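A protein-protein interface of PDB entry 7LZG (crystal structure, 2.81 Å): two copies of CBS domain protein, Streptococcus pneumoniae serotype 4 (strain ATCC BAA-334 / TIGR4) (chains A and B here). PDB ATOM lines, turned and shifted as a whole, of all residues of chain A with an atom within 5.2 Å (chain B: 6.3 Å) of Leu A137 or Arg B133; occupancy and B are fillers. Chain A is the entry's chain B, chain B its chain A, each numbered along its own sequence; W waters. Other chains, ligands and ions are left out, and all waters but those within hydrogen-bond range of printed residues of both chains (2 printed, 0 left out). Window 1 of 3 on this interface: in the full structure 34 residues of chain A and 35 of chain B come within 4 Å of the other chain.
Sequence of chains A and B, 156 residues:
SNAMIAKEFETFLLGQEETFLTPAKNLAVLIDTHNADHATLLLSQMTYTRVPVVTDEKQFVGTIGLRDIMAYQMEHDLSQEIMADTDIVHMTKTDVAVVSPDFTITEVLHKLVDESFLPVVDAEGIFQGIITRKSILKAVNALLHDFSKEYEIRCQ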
ATOM      1  N   THR A 132      22.232  33.224  -1.799  1.00  0.00           N
ATOM      2  CA  THR A 132      23.185  32.355  -2.468  1.00  0.00           C
ATOM      3  C   THR A 132      22.737  32.077  -3.897  1.00  0.00           C
ATOM      4  O   THR A 132      21.571  32.267  -4.254  1.00  0.00           O
ATOM      5  CB  THR A 132      23.356  31.029  -1.713  1.00  0.00           C
ATOM      6  OG1 THR A 132      22.099  30.346  -1.646  1.00  0.00           O
ATOM      7  CG2 THR A 132      23.858  31.286  -0.303  1.00  0.00           C
ATOM      8  N   ARG A 133      23.689  31.629  -4.721  1.00  0.00           N
ATOM      9  CA  ARG A 133      23.340  31.183  -6.066  1.00  0.00           C
ATOM     10  C   ARG A 133      22.357  30.023  -6.012  1.00  0.00           C
ATOM     11  O   ARG A 133      21.431  29.941  -6.829  1.00  0.00           O
ATOM     12  CB  ARG A 133      24.595  30.769  -6.834  1.00  0.00           C
ATOM     13  CG  ARG A 133      25.652  31.845  -6.986  1.00  0.00           C
ATOM     14  CD  ARG A 133      26.576  31.495  -8.142  1.00  0.00           C
ATOM     15  NE  ARG A 133      27.757  32.347  -8.214  1.00  0.00           N
ATOM     16  CZ  ARG A 133      29.005  31.906  -8.128  1.00  0.00           C
ATOM     17  NH1 ARG A 133      29.274  30.622  -7.962  1.00  0.00           N
ATOM     18  NH2 ARG A 133      30.007  32.775  -8.221  1.00  0.00           N
ATOM     19  N   LYS A 134      22.551  29.111  -5.057  1.00  0.00           N
ATOM     20  CA  LYS A 134      21.613  28.012  -4.865  1.00  0.00           C
ATOM     21  C   LYS A 134      20.213  28.530  -4.567  1.00  0.00           C
ATOM     22  O   LYS A 134      19.222  28.000  -5.081  1.00  0.00           O
ATOM     23  CB  LYS A 134      22.106  27.108  -3.735  1.00  0.00           C
ATOM     24  CG  LYS A 134      21.137  26.020  -3.312  1.00  0.00           C
ATOM     25  CD  LYS A 134      21.546  25.429  -1.971  1.00  0.00           C
ATOM     26  CE  LYS A 134      20.604  24.319  -1.537  1.00  0.00           C
ATOM     27  NZ  LYS A 134      20.699  23.127  -2.423  1.00  0.00           N
ATOM     28  N   SER A 135      20.114  29.577  -3.746  1.00  0.00           N
ATOM     29  CA  SER A 135      18.805  30.086  -3.352  1.00  0.00           C
ATOM     30  C   SER A 135      18.115  30.801  -4.507  1.00  0.00           C
ATOM     31  O   SER A 135      16.886  30.740  -4.637  1.00  0.00           O
ATOM     32  CB  SER A 135      18.951  31.014  -2.148  1.00  0.00           C
ATOM     33  OG  SER A 135      19.837  32.082  -2.425  1.00  0.00           O
ATOM     34  N   ILE A 136      18.884  31.484  -5.355  1.00  0.00           N
ATOM     35  CA  ILE A 136      18.294  32.151  -6.510  1.00  0.00           C
ATOM     36  C   ILE A 136      17.840  31.128  -7.541  1.00  0.00           C
ATOM     37  O   ILE A 136      16.784  31.285  -8.169  1.00  0.00           O
ATOM     38  CB  ILE A 136      19.287  33.169  -7.104  1.00  0.00           C
ATOM     39  CG1 ILE A 136      19.159  34.505  -6.373  1.00  0.00           C
ATOM     40  CG2 ILE A 136      19.071  33.344  -8.602  1.00  0.00           C
ATOM     41  CD1 ILE A 136      19.830  35.660  -7.074  1.00  0.00           C
ATOM     42  N   LEU A 137      18.617  30.058  -7.725  1.00  0.00           N
ATOM     43  CA  LEU A 137      18.186  28.993  -8.624  1.00  0.00           C
ATOM     44  C   LEU A 137      16.886  28.360  -8.152  1.00  0.00           C
ATOM     45  O   LEU A 137      16.071  27.934  -8.977  1.00  0.00           O
ATOM     46  CB  LEU A 137      19.277  27.934  -8.757  1.00  0.00           C
ATOM     47  CG  LEU A 137      20.245  28.173  -9.915  1.00  0.00           C
ATOM     48  CD1 LEU A 137      21.073  26.940 -10.158  1.00  0.00           C
ATOM     49  CD2 LEU A 137      19.483  28.551 -11.169  1.00  0.00           C
ATOM     50  N   LYS A 138      16.672  28.293  -6.836  1.00  0.00           N
ATOM     51  CA  LYS A 138      15.382  27.836  -6.331  1.00  0.00           C
ATOM     52  C   LYS A 138      14.268  28.786  -6.748  1.00  0.00           C
ATOM     53  O   LYS A 138      13.143  28.354  -7.023  1.00  0.00           O
ATOM     54  CB  LYS A 138      15.423  27.694  -4.810  1.00  0.00           C
ATOM     55  CG  LYS A 138      16.062  26.409  -4.313  1.00  0.00           C
ATOM     56  CD  LYS A 138      15.763  26.184  -2.838  1.00  0.00           C
ATOM     57  CE  LYS A 138      16.301  24.844  -2.361  1.00  0.00           C
ATOM     58  NZ  LYS A 138      15.938  24.574  -0.942  1.00  0.00           N
ATOM     59  N   ALA A 139      14.568  30.086  -6.810  1.00  0.00           N
ATOM     60  CA  ALA A 139      13.555  31.064  -7.187  1.00  0.00           C
ATOM     61  C   ALA A 139      13.155  30.901  -8.647  1.00  0.00           C
ATOM     62  O   ALA A 139      11.962  30.873  -8.973  1.00  0.00           O
ATOM     63  CB  ALA A 139      14.064  32.480  -6.920  1.00  0.00           C
ATOM     64  N   VAL A 140      14.138  30.792  -9.544  1.00  0.00           N
ATOM     65  CA  VAL A 140      13.834  30.613 -10.959  1.00  0.00           C
ATOM     66  C   VAL A 140      13.331  29.214 -11.272  1.00  0.00           C
ATOM     67  O   VAL A 140      12.766  28.997 -12.350  1.00  0.00           O
ATOM     68  CB  VAL A 140      15.063  30.932 -11.833  1.00  0.00           C
ATOM     69  CG1 VAL A 140      15.604  32.314 -11.502  1.00  0.00           C
ATOM     70  CG2 VAL A 140      16.134  29.870 -11.658  1.00  0.00           C
ATOM     71  N   ASN A 141      13.519  28.257 -10.360  1.00  0.00           N
ATOM     72  CA  ASN A 141      12.928  26.938 -10.545  1.00  0.00           C
ATOM     73  C   ASN A 141      11.420  26.941 -10.336  1.00  0.00           C
ATOM     74  O   ASN A 141      10.770  25.934 -10.635  1.00  0.00           O
ATOM     75  CB  ASN A 141      13.586  25.925  -9.607  1.00  0.00           C
ATOM     76  CG  ASN A 141      14.781  25.241 -10.241  1.00  0.00           C
ATOM     77  OD1 ASN A 141      14.662  24.142 -10.784  1.00  0.00           O
ATOM     78  ND2 ASN A 141      15.937  25.892 -10.188  1.00  0.00           N
ATOM     79  N   VAL B 108      19.202  20.817 -16.505  1.00  0.00           N
ATOM     80  CA  VAL B 108      20.287  21.610 -15.928  1.00  0.00           C
ATOM     81  C   VAL B 108      19.792  22.382 -14.709  1.00  0.00           C
ATOM     82  O   VAL B 108      20.311  22.225 -13.599  1.00  0.00           O
ATOM     83  CB  VAL B 108      20.887  22.553 -16.984  1.00  0.00           C
ATOM     84  CG1 VAL B 108      21.969  23.422 -16.363  1.00  0.00           C
ATOM     85  CG2 VAL B 108      21.445  21.756 -18.151  1.00  0.00           C
ATOM     86  N   LEU B 109      18.775  23.225 -14.903  1.00  0.00           N
ATOM     87  CA  LEU B 109      18.291  24.064 -13.812  1.00  0.00           C
ATOM     88  C   LEU B 109      17.708  23.236 -12.675  1.00  0.00           C
ATOM     89  O   LEU B 109      17.771  23.650 -11.512  1.00  0.00           O
ATOM     90  CB  LEU B 109      17.249  25.056 -14.331  1.00  0.00           C
ATOM     91  CG  LEU B 109      17.748  26.396 -14.876  1.00  0.00           C
ATOM     92  CD1 LEU B 109      18.706  26.213 -16.043  1.00  0.00           C
ATOM     93  CD2 LEU B 109      16.567  27.261 -15.285  1.00  0.00           C
ATOM     94  N   LEU B 112      20.786  21.479 -10.886  1.00  0.00           N
ATOM     95  CA  LEU B 112      21.658  22.474 -10.273  1.00  0.00           C
ATOM     96  C   LEU B 112      21.119  23.004  -8.952  1.00  0.00           C
ATOM     97  O   LEU B 112      21.784  23.839  -8.327  1.00  0.00           O
ATOM     98  CB  LEU B 112      21.890  23.641 -11.233  1.00  0.00           C
ATOM     99  CG  LEU B 112      23.030  23.501 -12.242  1.00  0.00           C
ATOM    100  CD1 LEU B 112      23.135  24.757 -13.090  1.00  0.00           C
ATOM    101  CD2 LEU B 112      24.345  23.223 -11.530  1.00  0.00           C
ATOM    102  N   VAL B 113      19.944  22.556  -8.515  1.00  0.00           N
ATOM    103  CA  VAL B 113      19.446  22.972  -7.211  1.00  0.00           C
ATOM    104  C   VAL B 113      20.184  22.242  -6.093  1.00  0.00           C
ATOM    105  O   VAL B 113      20.408  22.809  -5.019  1.00  0.00           O
ATOM    106  CB  VAL B 113      17.927  22.750  -7.125  1.00  0.00           C
ATOM    107  CG1 VAL B 113      17.387  23.245  -5.793  1.00  0.00           C
ATOM    108  CG2 VAL B 113      17.223  23.450  -8.275  1.00  0.00           C
ATOM    109  N   ASP B 114      20.592  20.994  -6.324  1.00  0.00           N
ATOM    110  CA  ASP B 114      21.199  20.189  -5.270  1.00  0.00           C
ATOM    111  C   ASP B 114      22.720  20.291  -5.245  1.00  0.00           C
ATOM    112  O   ASP B 114      23.315  20.331  -4.163  1.00  0.00           O
ATOM    113  CB  ASP B 114      20.781  18.726  -5.421  1.00  0.00           C
ATOM    114  CG  ASP B 114      19.286  18.532  -5.279  1.00  0.00           C
ATOM    115  OD1 ASP B 114      18.645  19.335  -4.569  1.00  0.00           O
ATOM    116  OD2 ASP B 114      18.752  17.574  -5.877  1.00  0.00           O
ATOM    117  N   GLU B 115      23.367  20.324  -6.407  1.00  0.00           N
ATOM    118  CA  GLU B 115      24.818  20.405  -6.481  1.00  0.00           C
ATOM    119  C   GLU B 115      25.240  21.714  -7.135  1.00  0.00           C
ATOM    120  O   GLU B 115      24.508  22.287  -7.949  1.00  0.00           O
ATOM    121  CB  GLU B 115      25.403  19.213  -7.248  1.00  0.00           C
ATOM    122  CG  GLU B 115      24.783  18.981  -8.612  1.00  0.00           C
ATOM    123  CD  GLU B 115      25.373  17.778  -9.321  1.00  0.00           C
ATOM    124  OE1 GLU B 115      26.238  17.098  -8.729  1.00  0.00           O
ATOM    125  OE2 GLU B 115      24.974  17.511 -10.472  1.00  0.00           O
ATOM    126  N   SER B 116      26.438  22.182  -6.769  1.00  0.00           N
ATOM    127  CA  SER B 116      26.915  23.485  -7.220  1.00  0.00           C
ATOM    128  C   SER B 116      27.341  23.483  -8.682  1.00  0.00           C
ATOM    129  O   SER B 116      27.338  24.544  -9.313  1.00  0.00           O
ATOM    130  CB  SER B 116      28.076  23.950  -6.343  1.00  0.00           C
ATOM    131  OG  SER B 116      29.135  23.011  -6.361  1.00  0.00           O
ATOM    132  N   PHE B 117      27.723  22.333  -9.229  1.00  0.00           N
ATOM    133  CA  PHE B 117      28.003  22.219 -10.652  1.00  0.00           C
ATOM    134  C   PHE B 117      27.525  20.860 -11.141  1.00  0.00           C
ATOM    135  O   PHE B 117      27.375  19.913 -10.367  1.00  0.00           O
ATOM    136  CB  PHE B 117      29.493  22.429 -10.974  1.00  0.00           C
ATOM    137  CG  PHE B 117      30.405  21.379 -10.399  1.00  0.00           C
ATOM    138  CD1 PHE B 117      30.684  20.217 -11.104  1.00  0.00           C
ATOM    139  CD2 PHE B 117      31.010  21.567  -9.168  1.00  0.00           C
ATOM    140  CE1 PHE B 117      31.528  19.257 -10.583  1.00  0.00           C
ATOM    141  CE2 PHE B 117      31.859  20.611  -8.643  1.00  0.00           C
ATOM    142  CZ  PHE B 117      32.119  19.455  -9.352  1.00  0.00           C
ATOM    143  N   LEU B 118      27.292  20.778 -12.446  1.00  0.00           N
ATOM    144  CA  LEU B 118      26.670  19.609 -13.056  1.00  0.00           C
ATOM    145  C   LEU B 118      27.680  18.869 -13.922  1.00  0.00           C
ATOM    146  O   LEU B 118      28.114  19.405 -14.953  1.00  0.00           O
ATOM    147  CB  LEU B 118      25.462  20.039 -13.889  1.00  0.00           C
ATOM    148  CG  LEU B 118      24.588  18.966 -14.532  1.00  0.00           C
ATOM    149  CD1 LEU B 118      24.018  18.034 -13.480  1.00  0.00           C
ATOM    150  CD2 LEU B 118      23.476  19.631 -15.321  1.00  0.00           C
ATOM    151  N   ILE B 131      28.859  21.847 -15.886  1.00  0.00           N
ATOM    152  CA  ILE B 131      28.012  23.025 -16.039  1.00  0.00           C
ATOM    153  C   ILE B 131      27.819  23.611 -14.650  1.00  0.00           C
ATOM    154  O   ILE B 131      27.191  22.985 -13.787  1.00  0.00           O
ATOM    155  CB  ILE B 131      26.664  22.692 -16.692  1.00  0.00           C
ATOM    156  CG1 ILE B 131      26.875  22.126 -18.097  1.00  0.00           C
ATOM    157  CG2 ILE B 131      25.780  23.926 -16.738  1.00  0.00           C
ATOM    158  CD1 ILE B 131      25.603  21.646 -18.756  1.00  0.00           C
ATOM    159  N   THR B 132      28.354  24.806 -14.426  1.00  0.00           N
ATOM    160  CA  THR B 132      28.373  25.398 -13.098  1.00  0.00           C
ATOM    161  C   THR B 132      27.149  26.275 -12.869  1.00  0.00           C
ATOM    162  O   THR B 132      26.547  26.797 -13.811  1.00  0.00           O
ATOM    163  CB  THR B 132      29.642  26.227 -12.894  1.00  0.00           C
ATOM    164  OG1 THR B 132      29.627  27.350 -13.785  1.00  0.00           O
ATOM    165  CG2 THR B 132      30.875  25.385 -13.175  1.00  0.00           C
ATOM    166  N   ARG B 133      26.781  26.426 -11.592  1.00  0.00           N
ATOM    167  CA  ARG B 133      25.748  27.389 -11.231  1.00  0.00           C
ATOM    168  C   ARG B 133      26.143  28.801 -11.636  1.00  0.00           C
ATOM    169  O   ARG B 133      25.276  29.624 -11.951  1.00  0.00           O
ATOM    170  CB  ARG B 133      25.472  27.338  -9.727  1.00  0.00           C
ATOM    171  CG  ARG B 133      24.564  26.205  -9.285  1.00  0.00           C
ATOM    172  CD  ARG B 133      23.804  26.583  -8.021  1.00  0.00           C
ATOM    173  NE  ARG B 133      24.639  26.560  -6.827  1.00  0.00           N
ATOM    174  CZ  ARG B 133      24.567  25.630  -5.886  1.00  0.00           C
ATOM    175  NH1 ARG B 133      23.694  24.640  -5.959  1.00  0.00           N
ATOM    176  NH2 ARG B 133      25.393  25.697  -4.845  1.00  0.00           N
ATOM    177  N   LYS B 134      27.444  29.099 -11.630  1.00  0.00           N
ATOM    178  CA  LYS B 134      27.915  30.421 -12.028  1.00  0.00           C
ATOM    179  C   LYS B 134      27.591  30.706 -13.490  1.00  0.00           C
ATOM    180  O   LYS B 134      27.255  31.840 -13.849  1.00  0.00           O
ATOM    181  CB  LYS B 134      29.419  30.523 -11.772  1.00  0.00           C
ATOM    182  CG  LYS B 134      30.041  31.874 -12.082  1.00  0.00           C
ATOM    183  CD  LYS B 134      31.529  31.843 -11.767  1.00  0.00           C
ATOM    184  CE  LYS B 134      32.204  33.171 -12.060  1.00  0.00           C
ATOM    185  NZ  LYS B 134      33.657  33.117 -11.737  1.00  0.00           N
ATOM    186  N   SER B 135      27.680  29.685 -14.346  1.00  0.00           N
ATOM    187  CA  SER B 135      27.396  29.881 -15.765  1.00  0.00           C
ATOM    188  C   SER B 135      25.924  30.196 -15.998  1.00  0.00           C
ATOM    189  O   SER B 135      25.592  31.071 -16.806  1.00  0.00           O
ATOM    190  CB  SER B 135      27.812  28.643 -16.559  1.00  0.00           C
ATOM    191  OG  SER B 135      29.196  28.373 -16.404  1.00  0.00           O
ATOM    192  N   ILE B 136      25.027  29.493 -15.303  1.00  0.00           N
ATOM    193  CA  ILE B 136      23.601  29.763 -15.454  1.00  0.00           C
ATOM    194  C   ILE B 136      23.261  31.149 -14.922  1.00  0.00           C
ATOM    195  O   ILE B 136      22.468  31.884 -15.523  1.00  0.00           O
ATOM    196  CB  ILE B 136      22.768  28.666 -14.760  1.00  0.00           C
ATOM    197  CG1 ILE B 136      22.396  27.560 -15.751  1.00  0.00           C
ATOM    198  CG2 ILE B 136      21.508  29.247 -14.138  1.00  0.00           C
ATOM    199  CD1 ILE B 136      23.576  26.807 -16.317  1.00  0.00           C
ATOM    200  N   LEU B 137      23.867  31.537 -13.797  1.00  0.00           N
ATOM    201  CA  LEU B 137      23.587  32.845 -13.221  1.00  0.00           C
ATOM    202  C   LEU B 137      24.137  33.979 -14.076  1.00  0.00           C
ATOM    203  O   LEU B 137      23.629  35.103 -13.992  1.00  0.00           O
ATOM    204  CB  LEU B 137      24.148  32.921 -11.800  1.00  0.00           C
ATOM    205  CG  LEU B 137      23.450  33.906 -10.862  1.00  0.00           C
ATOM    206  CD1 LEU B 137      23.281  33.290  -9.483  1.00  0.00           C
ATOM    207  CD2 LEU B 137      24.222  35.213 -10.774  1.00  0.00           C
ATOM    208  N   LYS B 138      25.158  33.712 -14.895  1.00  0.00           N
ATOM    209  CA  LYS B 138      25.609  34.709 -15.861  1.00  0.00           C
ATOM    210  C   LYS B 138      24.547  34.961 -16.923  1.00  0.00           C
ATOM    211  O   LYS B 138      24.357  36.103 -17.360  1.00  0.00           O
ATOM    212  CB  LYS B 138      26.923  34.265 -16.509  1.00  0.00           C
ATOM    213  CG  LYS B 138      28.167  34.518 -15.662  1.00  0.00           C
ATOM    214  CD  LYS B 138      29.445  34.085 -16.379  1.00  0.00           C
ATOM    215  CE  LYS B 138      30.028  32.811 -15.773  1.00  0.00           C
ATOM    216  NZ  LYS B 138      31.083  32.196 -16.631  1.00  0.00           N
ATOM    217  N   VAL B 140      21.245  34.446 -16.441  1.00  0.00           N
ATOM    218  CA  VAL B 140      20.155  35.114 -15.736  1.00  0.00           C
ATOM    219  C   VAL B 140      20.477  36.589 -15.536  1.00  0.00           C
ATOM    220  O   VAL B 140      19.588  37.448 -15.592  1.00  0.00           O
ATOM    221  CB  VAL B 140      19.875  34.410 -14.395  1.00  0.00           C
ATOM    222  CG1 VAL B 140      18.737  35.093 -13.659  1.00  0.00           C
ATOM    223  CG2 VAL B 140      19.560  32.942 -14.622  1.00  0.00           C
HETATM  224  O   HOH W   1      29.177  27.567  -9.179  1.00  0.00           O
HETATM  225  O   HOH W   2      25.587  28.599  -3.878  1.00  0.00           O
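Water W2 lies within hydrogen-bond range of the guanidinium group of Arg B133 (3.1 Å) and the backbone NH of Lys A134 (3.3 Å). Water W1 lies within hydrogen-bond range of the guanidinium group of Arg A133 (3.3 Å) and the backbone NH of Lys B134 (3.4 Å).
The backbone carbonyl oxygen of Ser B116 is in hydrogen-bond range of the backbone NH of Arg B133 (3.0 Å). NH1 of Arg B133 lies within hydrogen-bond range of O of Glu B115, 3.2 Å away. The guanidinium group (NH1) of Arg B133 sits at hydrogen-bond distance from the backbone carbonyl oxygen (O) of Leu B112, at 3.1 Å.
The backbone carbonyl oxygen (O) of Leu B109 sits at hydrogen-bond distance from the side-chain amide nitrogen (ND2) of Asn A141, 3.2 Å away. O of Val B113 is in hydrogen-bond range of NZ of Lys A134.
Printed residues of chain A that touch a printed residue of chain B: Arg A133, Lys A134, Leu A137, Lys A138 and Asn A141. Hydrophobic or aromatic side chains of chain A that line the printed part of chain B: Leu A137. Printed residues of chain B that touch a printed residue of chain A: Leu B109, Leu B112, Val B113, Arg B133, Lys B134, Ile B136 and Leu B137. Hydrophobic or aromatic side chains of chain B within 4 Å of the printed part of chain A: Leu B112, Val B113, Ile B136 and Leu B137. Among the printed residues, 10 pairs touch across the chains. Among the printed residues, no Asp or Glu carboxylate lies within 4 Å of a Lys or Arg side-chain nitrogen of the other chain.
Arg B133 touches just these residues of chain A: Lys A134 (3.6 Å) and Leu A137 (3.5 Å). Of the printed residues of chain B, Arg A133 touches Lys B134 (3.8 Å) and Leu B137 (3.7 Å). Of the printed residues of chain A, Ile B136 touches Leu A137 (3.7 Å). Of the printed residues of chain B, Asn A141 touches Leu B109 (3.2 Å) and Val B113 (3.4 Å). Glu B115 touches none of the printed residues of chain A. Val B140 touches none of the printed residues of chain A. The nearest residue of chain B that does not touch Leu A137 is Leu B109 (4.6 Å).
Lys B134 touches Arg A133. CG of Arg A133 touches CD1 of Leu B137, at 3.7 Å. Lys A134 touches Arg B133 (CB to CZ, 3.6 Å). CD1 of Leu A137 touches CB of Leu B112, at 3.6 Å. Leu A137 touches Arg B133 (CD1 to CD, 3.5 Å). Leu A137 touches Ile B136 (CD2 to CG2, 3.7 Å). Val B113 touches Lys A138 (CG1 to CG, 3.7 Å). Asn A141 touches Val B113 (ND2 to CG2, 3.4 Å).
Arg A133 touches Lys B134, and with the chains exchanged Lys A134 touches Arg B133. Arg A133 touches Leu B137, and with the chains exchanged Leu A137 touches Arg B133. Leu A137 touches Ile B136, but with the chains exchanged Ile A136 does not touch Leu B137 (4.3 Å). Positions printed for both chains: 132, 133, 134, 135, 136, 137, 138 and 140.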
